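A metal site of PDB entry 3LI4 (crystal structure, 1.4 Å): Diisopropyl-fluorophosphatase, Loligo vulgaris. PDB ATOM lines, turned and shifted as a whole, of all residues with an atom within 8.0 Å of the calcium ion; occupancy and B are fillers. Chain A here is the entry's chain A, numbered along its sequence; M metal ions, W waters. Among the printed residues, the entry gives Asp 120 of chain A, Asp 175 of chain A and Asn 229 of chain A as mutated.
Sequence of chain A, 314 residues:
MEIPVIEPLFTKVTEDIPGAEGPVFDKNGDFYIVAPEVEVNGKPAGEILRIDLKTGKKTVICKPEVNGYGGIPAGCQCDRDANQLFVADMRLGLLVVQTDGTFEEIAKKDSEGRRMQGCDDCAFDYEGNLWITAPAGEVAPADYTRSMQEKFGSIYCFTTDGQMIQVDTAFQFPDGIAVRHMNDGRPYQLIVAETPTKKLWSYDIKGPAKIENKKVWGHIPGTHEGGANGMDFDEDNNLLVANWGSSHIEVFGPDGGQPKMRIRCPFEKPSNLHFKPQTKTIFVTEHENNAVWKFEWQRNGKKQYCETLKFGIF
Within 4 Å of the calcium ion: Glu 21, Asp 120, Asp 175 and Asn 229.
Water W2 bridges the side-chain carboxylate (OD2) of Asp 175 and the side-chain carboxylate (OD2) of Asp 120. Water W3 lies within hydrogen-bond range of the side-chain carboxylate (OD2) of Asp 121 (2.6 Å), the backbone NH (N) of Gly 230 (3.4 Å) and the side-chain amide nitrogen (ND2) of Asn 272 (3.5 Å).
The calcium ion is bound by OD1 of Asp 175 (2.4 Å). OE2 of Glu 21 binds the calcium ion, at 2.4 Å. OD1 of Asp 120 is bound to the calcium ion (2.5 Å). OD1 of Asn 229 is bound to the calcium ion, at 2.5 Å. Water W3 is bound to the calcium ion. The calcium ion is bound by water W2, at 2.6 Å. Water W1 is bound to the calcium ion, at 2.6 Å.
The side-chain hydroxyl (OG1) of Thr 133 is in hydrogen-bond range of the backbone carbonyl oxygen (O) of Asp 175, at 2.7 Å. The side-chain carboxylate (OD2) of Asp 175 sits close to the side-chain hydroxyl (OG1) of Thr 195, 3.4 Å away. The side-chain carboxylate of Glu 21 sits at hydrogen-bond distance from the side-chain amide nitrogen of Asn 272. The backbone NH of Gly 75 is in hydrogen-bond range of the backbone carbonyl oxygen of Asp 120 (3.1 Å). The backbone NH (N) of Asp 120 lies within hydrogen-bond range of the backbone carbonyl oxygen (O) of Thr 133 (2.9 Å). ND2 of Asn 229 lies close to O of Ser 271 (3.5 Å). The backbone carbonyl oxygen (O) of Asn 229 is in hydrogen-bond range of the backbone NH (N) of Gly 176 (2.8 Å).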
ATOM      1  N   GLY A  19      28.300 -21.124  25.497  1.00  0.00           N
ATOM      2  CA  GLY A  19      26.973 -21.003  24.925  1.00  0.00           C
ATOM      3  C   GLY A  19      25.968 -20.404  25.893  1.00  0.00           C
ATOM      4  O   GLY A  19      24.760 -20.593  25.715  1.00  0.00           O
ATOM      5  N   ALA A  20      26.481 -19.680  26.894  1.00  0.00           N
ATOM      6  CA  ALA A  20      25.661 -19.026  27.918  1.00  0.00           C
ATOM      7  C   ALA A  20      24.234 -18.768  27.443  1.00  0.00           C
ATOM      8  O   ALA A  20      24.011 -18.033  26.489  1.00  0.00           O
ATOM      9  CB  ALA A  20      26.314 -17.718  28.349  1.00  0.00           C
ATOM     10  N   GLU A  21      23.277 -19.354  28.153  1.00  0.00           N
ATOM     11  CA  GLU A  21      21.874 -19.251  27.778  1.00  0.00           C
ATOM     12  C   GLU A  21      20.925 -19.422  28.958  1.00  0.00           C
ATOM     13  O   GLU A  21      21.351 -19.579  30.108  1.00  0.00           O
ATOM     14  CB  GLU A  21      21.560 -20.345  26.751  1.00  0.00           C
ATOM     15  CG  GLU A  21      21.471 -19.849  25.335  1.00  0.00           C
ATOM     16  CD  GLU A  21      20.107 -19.316  24.991  1.00  0.00           C
ATOM     17  OE1 GLU A  21      19.360 -18.919  25.901  1.00  0.00           O
ATOM     18  OE2 GLU A  21      19.785 -19.317  23.786  1.00  0.00           O
ATOM     19  N   GLY A  22      19.632 -19.375  28.647  1.00  0.00           N
ATOM     20  CA  GLY A  22      18.592 -19.590  29.626  1.00  0.00           C
ATOM     21  C   GLY A  22      18.702 -19.025  31.028  1.00  0.00           C
ATOM     22  O   GLY A  22      18.579 -19.778  31.996  1.00  0.00           O
ATOM     23  N   PRO A  36      24.828 -24.766  27.208  1.00  0.00           N
ATOM     24  CA  PRO A  36      24.519 -25.802  26.224  1.00  0.00           C
ATOM     25  C   PRO A  36      25.694 -26.334  25.413  1.00  0.00           C
ATOM     26  O   PRO A  36      25.684 -27.497  24.994  1.00  0.00           O
ATOM     27  CB  PRO A  36      23.486 -25.126  25.319  1.00  0.00           C
ATOM     28  CG  PRO A  36      23.832 -23.661  25.425  1.00  0.00           C
ATOM     29  CD  PRO A  36      24.130 -23.511  26.895  1.00  0.00           C
ATOM     30  N   ALA A  74      19.243 -25.409  26.875  1.00  0.00           N
ATOM     31  CA  ALA A  74      19.282 -24.087  26.283  1.00  0.00           C
ATOM     32  C   ALA A  74      18.349 -23.018  26.818  1.00  0.00           C
ATOM     33  O   ALA A  74      18.600 -21.828  26.623  1.00  0.00           O
ATOM     34  CB  ALA A  74      19.071 -24.231  24.781  1.00  0.00           C
ATOM     35  N   GLY A  75      17.264 -23.414  27.469  1.00  0.00           N
ATOM     36  CA  GLY A  75      16.321 -22.426  27.979  1.00  0.00           C
ATOM     37  C   GLY A  75      15.613 -22.893  29.226  1.00  0.00           C
ATOM     38  O   GLY A  75      15.404 -24.093  29.424  1.00  0.00           O
ATOM     39  N   MET A  90      18.128 -29.073  23.615  1.00  0.00           N
ATOM     40  CA  MET A  90      18.194 -29.349  22.188  1.00  0.00           C
ATOM     41  C   MET A  90      18.399 -30.813  21.824  1.00  0.00           C
ATOM     42  O   MET A  90      18.119 -31.213  20.693  1.00  0.00           O
ATOM     43  CB  MET A  90      19.276 -28.485  21.538  1.00  0.00           C
ATOM     44  CG  MET A  90      18.924 -26.996  21.478  1.00  0.00           C
ATOM     45  SD  MET A  90      17.635 -26.602  20.269  1.00  0.00           S
ATOM     46  CE  MET A  90      18.618 -26.508  18.775  1.00  0.00           C
ATOM     47  N   CYS A 119      14.330 -29.103  22.121  1.00  0.00           N
ATOM     48  CA  CYS A 119      13.784 -27.793  22.419  1.00  0.00           C
ATOM     49  C   CYS A 119      14.831 -26.736  22.733  1.00  0.00           C
ATOM     50  O   CYS A 119      15.940 -27.060  23.149  1.00  0.00           O
ATOM     51  CB  CYS A 119      12.779 -27.920  23.570  1.00  0.00           C
ATOM     52  SG  CYS A 119      11.419 -29.022  23.135  1.00  0.00           S
ATOM     53  N   ASP A 120      14.448 -25.474  22.558  1.00  0.00           N
ATOM     54  CA  ASP A 120      15.356 -24.373  22.767  1.00  0.00           C
ATOM     55  C   ASP A 120      14.965 -23.423  23.896  1.00  0.00           C
ATOM     56  O   ASP A 120      15.778 -23.089  24.746  1.00  0.00           O
ATOM     57  CB  ASP A 120      15.507 -23.620  21.452  1.00  0.00           C
ATOM     58  CG  ASP A 120      16.601 -22.597  21.495  1.00  0.00           C
ATOM     59  OD1 ASP A 120      16.450 -21.654  22.278  1.00  0.00           O
ATOM     60  OD2 ASP A 120      17.608 -22.738  20.766  1.00  0.00           O
ATOM     61  N   ASP A 121      13.728 -22.960  23.911  1.00  0.00           N
ATOM     62  CA  ASP A 121      13.288 -22.065  24.978  1.00  0.00           C
ATOM     63  C   ASP A 121      11.827 -22.347  25.290  1.00  0.00           C
ATOM     64  O   ASP A 121      11.147 -23.054  24.558  1.00  0.00           O
ATOM     65  CB  ASP A 121      13.477 -20.590  24.565  1.00  0.00           C
ATOM     66  CG  ASP A 121      13.813 -19.681  25.745  1.00  0.00           C
ATOM     67  OD1 ASP A 121      13.628 -20.104  26.901  1.00  0.00           O
ATOM     68  OD2 ASP A 121      14.245 -18.532  25.517  1.00  0.00           O
ATOM     69  N   CYS A 122      11.355 -21.797  26.407  1.00  0.00           N
ATOM     70  CA  CYS A 122       9.974 -22.008  26.795  1.00  0.00           C
ATOM     71  C   CYS A 122       9.461 -20.852  27.624  1.00  0.00           C
ATOM     72  O   CYS A 122      10.229 -20.057  28.177  1.00  0.00           O
ATOM     73  CB  CYS A 122       9.836 -23.331  27.554  1.00  0.00           C
ATOM     74  SG  CYS A 122      10.916 -23.535  29.011  1.00  0.00           S
ATOM     75  N   THR A 133       9.629 -23.837  22.156  1.00  0.00           N
ATOM     76  CA  THR A 133      10.112 -23.815  20.790  1.00  0.00           C
ATOM     77  C   THR A 133      11.001 -25.050  20.619  1.00  0.00           C
ATOM     78  O   THR A 133      11.749 -25.412  21.540  1.00  0.00           O
ATOM     79  CB  THR A 133      10.922 -22.549  20.469  1.00  0.00           C
ATOM     80  OG1 THR A 133      11.980 -22.393  21.420  1.00  0.00           O
ATOM     81  CG2 THR A 133      10.030 -21.320  20.489  1.00  0.00           C
ATOM     82  N   PRO A 135      13.468 -26.065  17.713  1.00  0.00           N
ATOM     83  CA  PRO A 135      14.174 -25.879  16.448  1.00  0.00           C
ATOM     84  C   PRO A 135      15.043 -27.060  16.023  1.00  0.00           C
ATOM     85  O   PRO A 135      15.505 -27.113  14.889  1.00  0.00           O
ATOM     86  CB  PRO A 135      14.993 -24.626  16.700  1.00  0.00           C
ATOM     87  CG  PRO A 135      15.352 -24.769  18.166  1.00  0.00           C
ATOM     88  CD  PRO A 135      14.070 -25.253  18.792  1.00  0.00           C
ATOM     89  N   PHE A 173      13.948 -22.491  12.527  1.00  0.00           N
ATOM     90  CA  PHE A 173      14.601 -22.217  13.802  1.00  0.00           C
ATOM     91  C   PHE A 173      13.838 -21.308  14.761  1.00  0.00           C
ATOM     92  O   PHE A 173      14.193 -20.136  14.956  1.00  0.00           O
ATOM     93  CB  PHE A 173      16.020 -21.696  13.612  1.00  0.00           C
ATOM     94  CG  PHE A 173      16.942 -22.069  14.738  1.00  0.00           C
ATOM     95  CD1 PHE A 173      16.915 -21.377  15.945  1.00  0.00           C
ATOM     96  CD2 PHE A 173      17.777 -23.173  14.626  1.00  0.00           C
ATOM     97  CE1 PHE A 173      17.707 -21.776  17.017  1.00  0.00           C
ATOM     98  CE2 PHE A 173      18.571 -23.583  15.690  1.00  0.00           C
ATOM     99  CZ  PHE A 173      18.532 -22.884  16.896  1.00  0.00           C
ATOM    100  N   PRO A 174      12.756 -21.830  15.342  1.00  0.00           N
ATOM    101  CA  PRO A 174      11.959 -21.063  16.302  1.00  0.00           C
ATOM    102  C   PRO A 174      12.881 -20.998  17.521  1.00  0.00           C
ATOM    103  O   PRO A 174      13.484 -22.001  17.908  1.00  0.00           O
ATOM    104  CB  PRO A 174      10.730 -21.935  16.511  1.00  0.00           C
ATOM    105  CG  PRO A 174      11.240 -23.324  16.249  1.00  0.00           C
ATOM    106  CD  PRO A 174      12.143 -23.138  15.058  1.00  0.00           C
ATOM    107  N   ASP A 175      13.001 -19.819  18.112  1.00  0.00           N
ATOM    108  CA  ASP A 175      13.918 -19.641  19.221  1.00  0.00           C
ATOM    109  C   ASP A 175      13.255 -19.073  20.476  1.00  0.00           C
ATOM    110  O   ASP A 175      12.695 -19.823  21.278  1.00  0.00           O
ATOM    111  CB  ASP A 175      15.065 -18.753  18.768  1.00  0.00           C
ATOM    112  CG  ASP A 175      16.308 -18.962  19.571  1.00  0.00           C
ATOM    113  OD1 ASP A 175      16.138 -19.151  20.776  1.00  0.00           O
ATOM    114  OD2 ASP A 175      17.429 -18.943  19.024  1.00  0.00           O
ATOM    115  N   GLY A 176      13.317 -17.760  20.653  1.00  0.00           N
ATOM    116  CA  GLY A 176      12.692 -17.161  21.815  1.00  0.00           C
ATOM    117  C   GLY A 176      11.183 -17.318  21.742  1.00  0.00           C
ATOM    118  O   GLY A 176      10.614 -17.487  20.667  1.00  0.00           O
ATOM    119  N   ILE A 177      10.531 -17.228  22.900  1.00  0.00           N
ATOM    120  CA  ILE A 177       9.088 -17.365  22.981  1.00  0.00           C
ATOM    121  C   ILE A 177       8.626 -16.628  24.235  1.00  0.00           C
ATOM    122  O   ILE A 177       9.339 -16.576  25.234  1.00  0.00           O
ATOM    123  CB  ILE A 177       8.710 -18.861  23.018  1.00  0.00           C
ATOM    124  CG1 ILE A 177       7.190 -19.032  23.000  1.00  0.00           C
ATOM    125  CG2 ILE A 177       9.332 -19.538  24.226  1.00  0.00           C
ATOM    126  CD1 ILE A 177       6.746 -20.433  22.553  1.00  0.00           C
ATOM    127  N   THR A 195      14.514 -17.062  14.188  1.00  0.00           N
ATOM    128  CA  THR A 195      15.821 -16.446  14.038  1.00  0.00           C
ATOM    129  C   THR A 195      16.343 -15.966  12.677  1.00  0.00           C
ATOM    130  O   THR A 195      16.434 -14.767  12.444  1.00  0.00           O
ATOM    131  CB  THR A 195      16.916 -17.305  14.700  1.00  0.00           C
ATOM    132  OG1 THR A 195      16.544 -17.588  16.057  1.00  0.00           O
ATOM    133  CG2 THR A 195      18.251 -16.557  14.697  1.00  0.00           C
ATOM    134  N   ALA A 228      16.674 -12.732  16.212  1.00  0.00           N
ATOM    135  CA  ALA A 228      16.047 -12.853  17.522  1.00  0.00           C
ATOM    136  C   ALA A 228      16.330 -14.174  18.201  1.00  0.00           C
ATOM    137  O   ALA A 228      16.122 -15.244  17.640  1.00  0.00           O
ATOM    138  CB  ALA A 228      14.534 -12.657  17.402  1.00  0.00           C
ATOM    139  N   ASN A 229      16.819 -14.081  19.429  1.00  0.00           N
ATOM    140  CA  ASN A 229      17.116 -15.258  20.220  1.00  0.00           C
ATOM    141  C   ASN A 229      16.109 -15.250  21.392  1.00  0.00           C
ATOM    142  O   ASN A 229      14.927 -15.470  21.178  1.00  0.00           O
ATOM    143  CB  ASN A 229      18.579 -15.219  20.711  1.00  0.00           C
ATOM    144  CG  ASN A 229      19.057 -16.571  21.188  1.00  0.00           C
ATOM    145  OD1 ASN A 229      18.331 -17.290  21.845  1.00  0.00           O
ATOM    146  ND2 ASN A 229      20.315 -16.923  20.865  1.00  0.00           N
ATOM    147  N   GLY A 230      16.561 -14.954  22.610  1.00  0.00           N
ATOM    148  CA  GLY A 230      15.656 -14.937  23.753  1.00  0.00           C
ATOM    149  C   GLY A 230      14.835 -13.665  23.907  1.00  0.00           C
ATOM    150  O   GLY A 230      15.202 -12.612  23.374  1.00  0.00           O
ATOM    151  N   MET A 231      13.746 -13.736  24.660  1.00  0.00           N
ATOM    152  CA  MET A 231      12.888 -12.577  24.848  1.00  0.00           C
ATOM    153  C   MET A 231      12.082 -12.615  26.146  1.00  0.00           C
ATOM    154  O   MET A 231      11.883 -13.674  26.741  1.00  0.00           O
ATOM    155  CB  MET A 231      11.891 -12.489  23.688  1.00  0.00           C
ATOM    156  CG  MET A 231      10.951 -13.692  23.635  1.00  0.00           C
ATOM    157  SD  MET A 231       9.643 -13.593  22.411  1.00  0.00           S
ATOM    158  CE  MET A 231      10.630 -13.350  20.971  1.00  0.00           C
ATOM    159  N   TRP A 244      20.735 -11.463  18.443  1.00  0.00           N
ATOM    160  CA  TRP A 244      22.035 -12.108  18.308  1.00  0.00           C
ATOM    161  C   TRP A 244      22.761 -11.659  17.039  1.00  0.00           C
ATOM    162  O   TRP A 244      22.244 -11.805  15.938  1.00  0.00           O
ATOM    163  CB  TRP A 244      21.825 -13.624  18.291  1.00  0.00           C
ATOM    164  CG  TRP A 244      23.039 -14.453  18.555  1.00  0.00           C
ATOM    165  CD1 TRP A 244      23.418 -14.983  19.765  1.00  0.00           C
ATOM    166  CD2 TRP A 244      23.985 -14.934  17.601  1.00  0.00           C
ATOM    167  NE1 TRP A 244      24.534 -15.768  19.606  1.00  0.00           N
ATOM    168  CE2 TRP A 244      24.906 -15.754  18.290  1.00  0.00           C
ATOM    169  CE3 TRP A 244      24.134 -14.758  16.213  1.00  0.00           C
ATOM    170  CZ2 TRP A 244      25.964 -16.401  17.639  1.00  0.00           C
ATOM    171  CZ3 TRP A 244      25.199 -15.390  15.579  1.00  0.00           C
ATOM    172  CH2 TRP A 244      26.098 -16.202  16.288  1.00  0.00           C
ATOM    173  N   SER A 271      22.316 -13.393  23.777  1.00  0.00           N
ATOM    174  CA  SER A 271      21.558 -14.599  23.466  1.00  0.00           C
ATOM    175  C   SER A 271      20.227 -14.677  24.189  1.00  0.00           C
ATOM    176  O   SER A 271      19.238 -15.131  23.635  1.00  0.00           O
ATOM    177  CB  SER A 271      22.384 -15.839  23.774  1.00  0.00           C
ATOM    178  OG  SER A 271      22.732 -15.892  25.148  1.00  0.00           O
ATOM    179  N   ASN A 272      20.194 -14.251  25.444  1.00  0.00           N
ATOM    180  CA  ASN A 272      18.959 -14.314  26.188  1.00  0.00           C
ATOM    181  C   ASN A 272      19.005 -13.333  27.350  1.00  0.00           C
ATOM    182  O   ASN A 272      20.048 -12.733  27.618  1.00  0.00           O
ATOM    183  CB  ASN A 272      18.725 -15.739  26.701  1.00  0.00           C
ATOM    184  CG  ASN A 272      17.265 -16.134  26.679  1.00  0.00           C
ATOM    185  OD1 ASN A 272      16.385 -15.300  26.907  1.00  0.00           O
ATOM    186  ND2 ASN A 272      16.981 -17.407  26.402  1.00  0.00           N
ATOM    187  N   THR A 285      22.711 -13.033  28.871  1.00  0.00           N
ATOM    188  CA  THR A 285      23.715 -14.011  28.513  1.00  0.00           C
ATOM    189  C   THR A 285      24.174 -13.627  27.106  1.00  0.00           C
ATOM    190  O   THR A 285      23.386 -13.098  26.321  1.00  0.00           O
ATOM    191  CB  THR A 285      23.140 -15.444  28.513  1.00  0.00           C
ATOM    192  OG1 THR A 285      21.922 -15.471  27.751  1.00  0.00           O
ATOM    193  CG2 THR A 285      22.843 -15.900  29.924  1.00  0.00           C
ATOM    194  N   HIS A 287      27.145 -14.635  23.708  1.00  0.00           N
ATOM    195  CA  HIS A 287      28.112 -15.554  23.123  1.00  0.00           C
ATOM    196  C   HIS A 287      29.401 -14.985  22.579  1.00  0.00           C
ATOM    197  O   HIS A 287      30.216 -15.731  22.039  1.00  0.00           O
ATOM    198  CB  HIS A 287      27.410 -16.372  22.046  1.00  0.00           C
ATOM    199  CG  HIS A 287      26.254 -17.163  22.559  1.00  0.00           C
ATOM    200  ND1 HIS A 287      25.281 -17.692  21.733  1.00  0.00           N
ATOM    201  CD2 HIS A 287      25.918 -17.527  23.818  1.00  0.00           C
ATOM    202  CE1 HIS A 287      24.397 -18.353  22.458  1.00  0.00           C
ATOM    203  NE2 HIS A 287      24.765 -18.272  23.728  1.00  0.00           N
HETATM  204 CA    CA M   1      17.613 -19.512  22.685  1.00  0.00          CA
HETATM  205  O   HOH W   1      16.898 -20.566  24.918  1.00  0.00           O
HETATM  206  O   HOH W   2      19.045 -20.233  20.694  1.00  0.00           O
HETATM  207  O   HOH W   3      15.618 -18.153  23.321  1.00  0.00           O
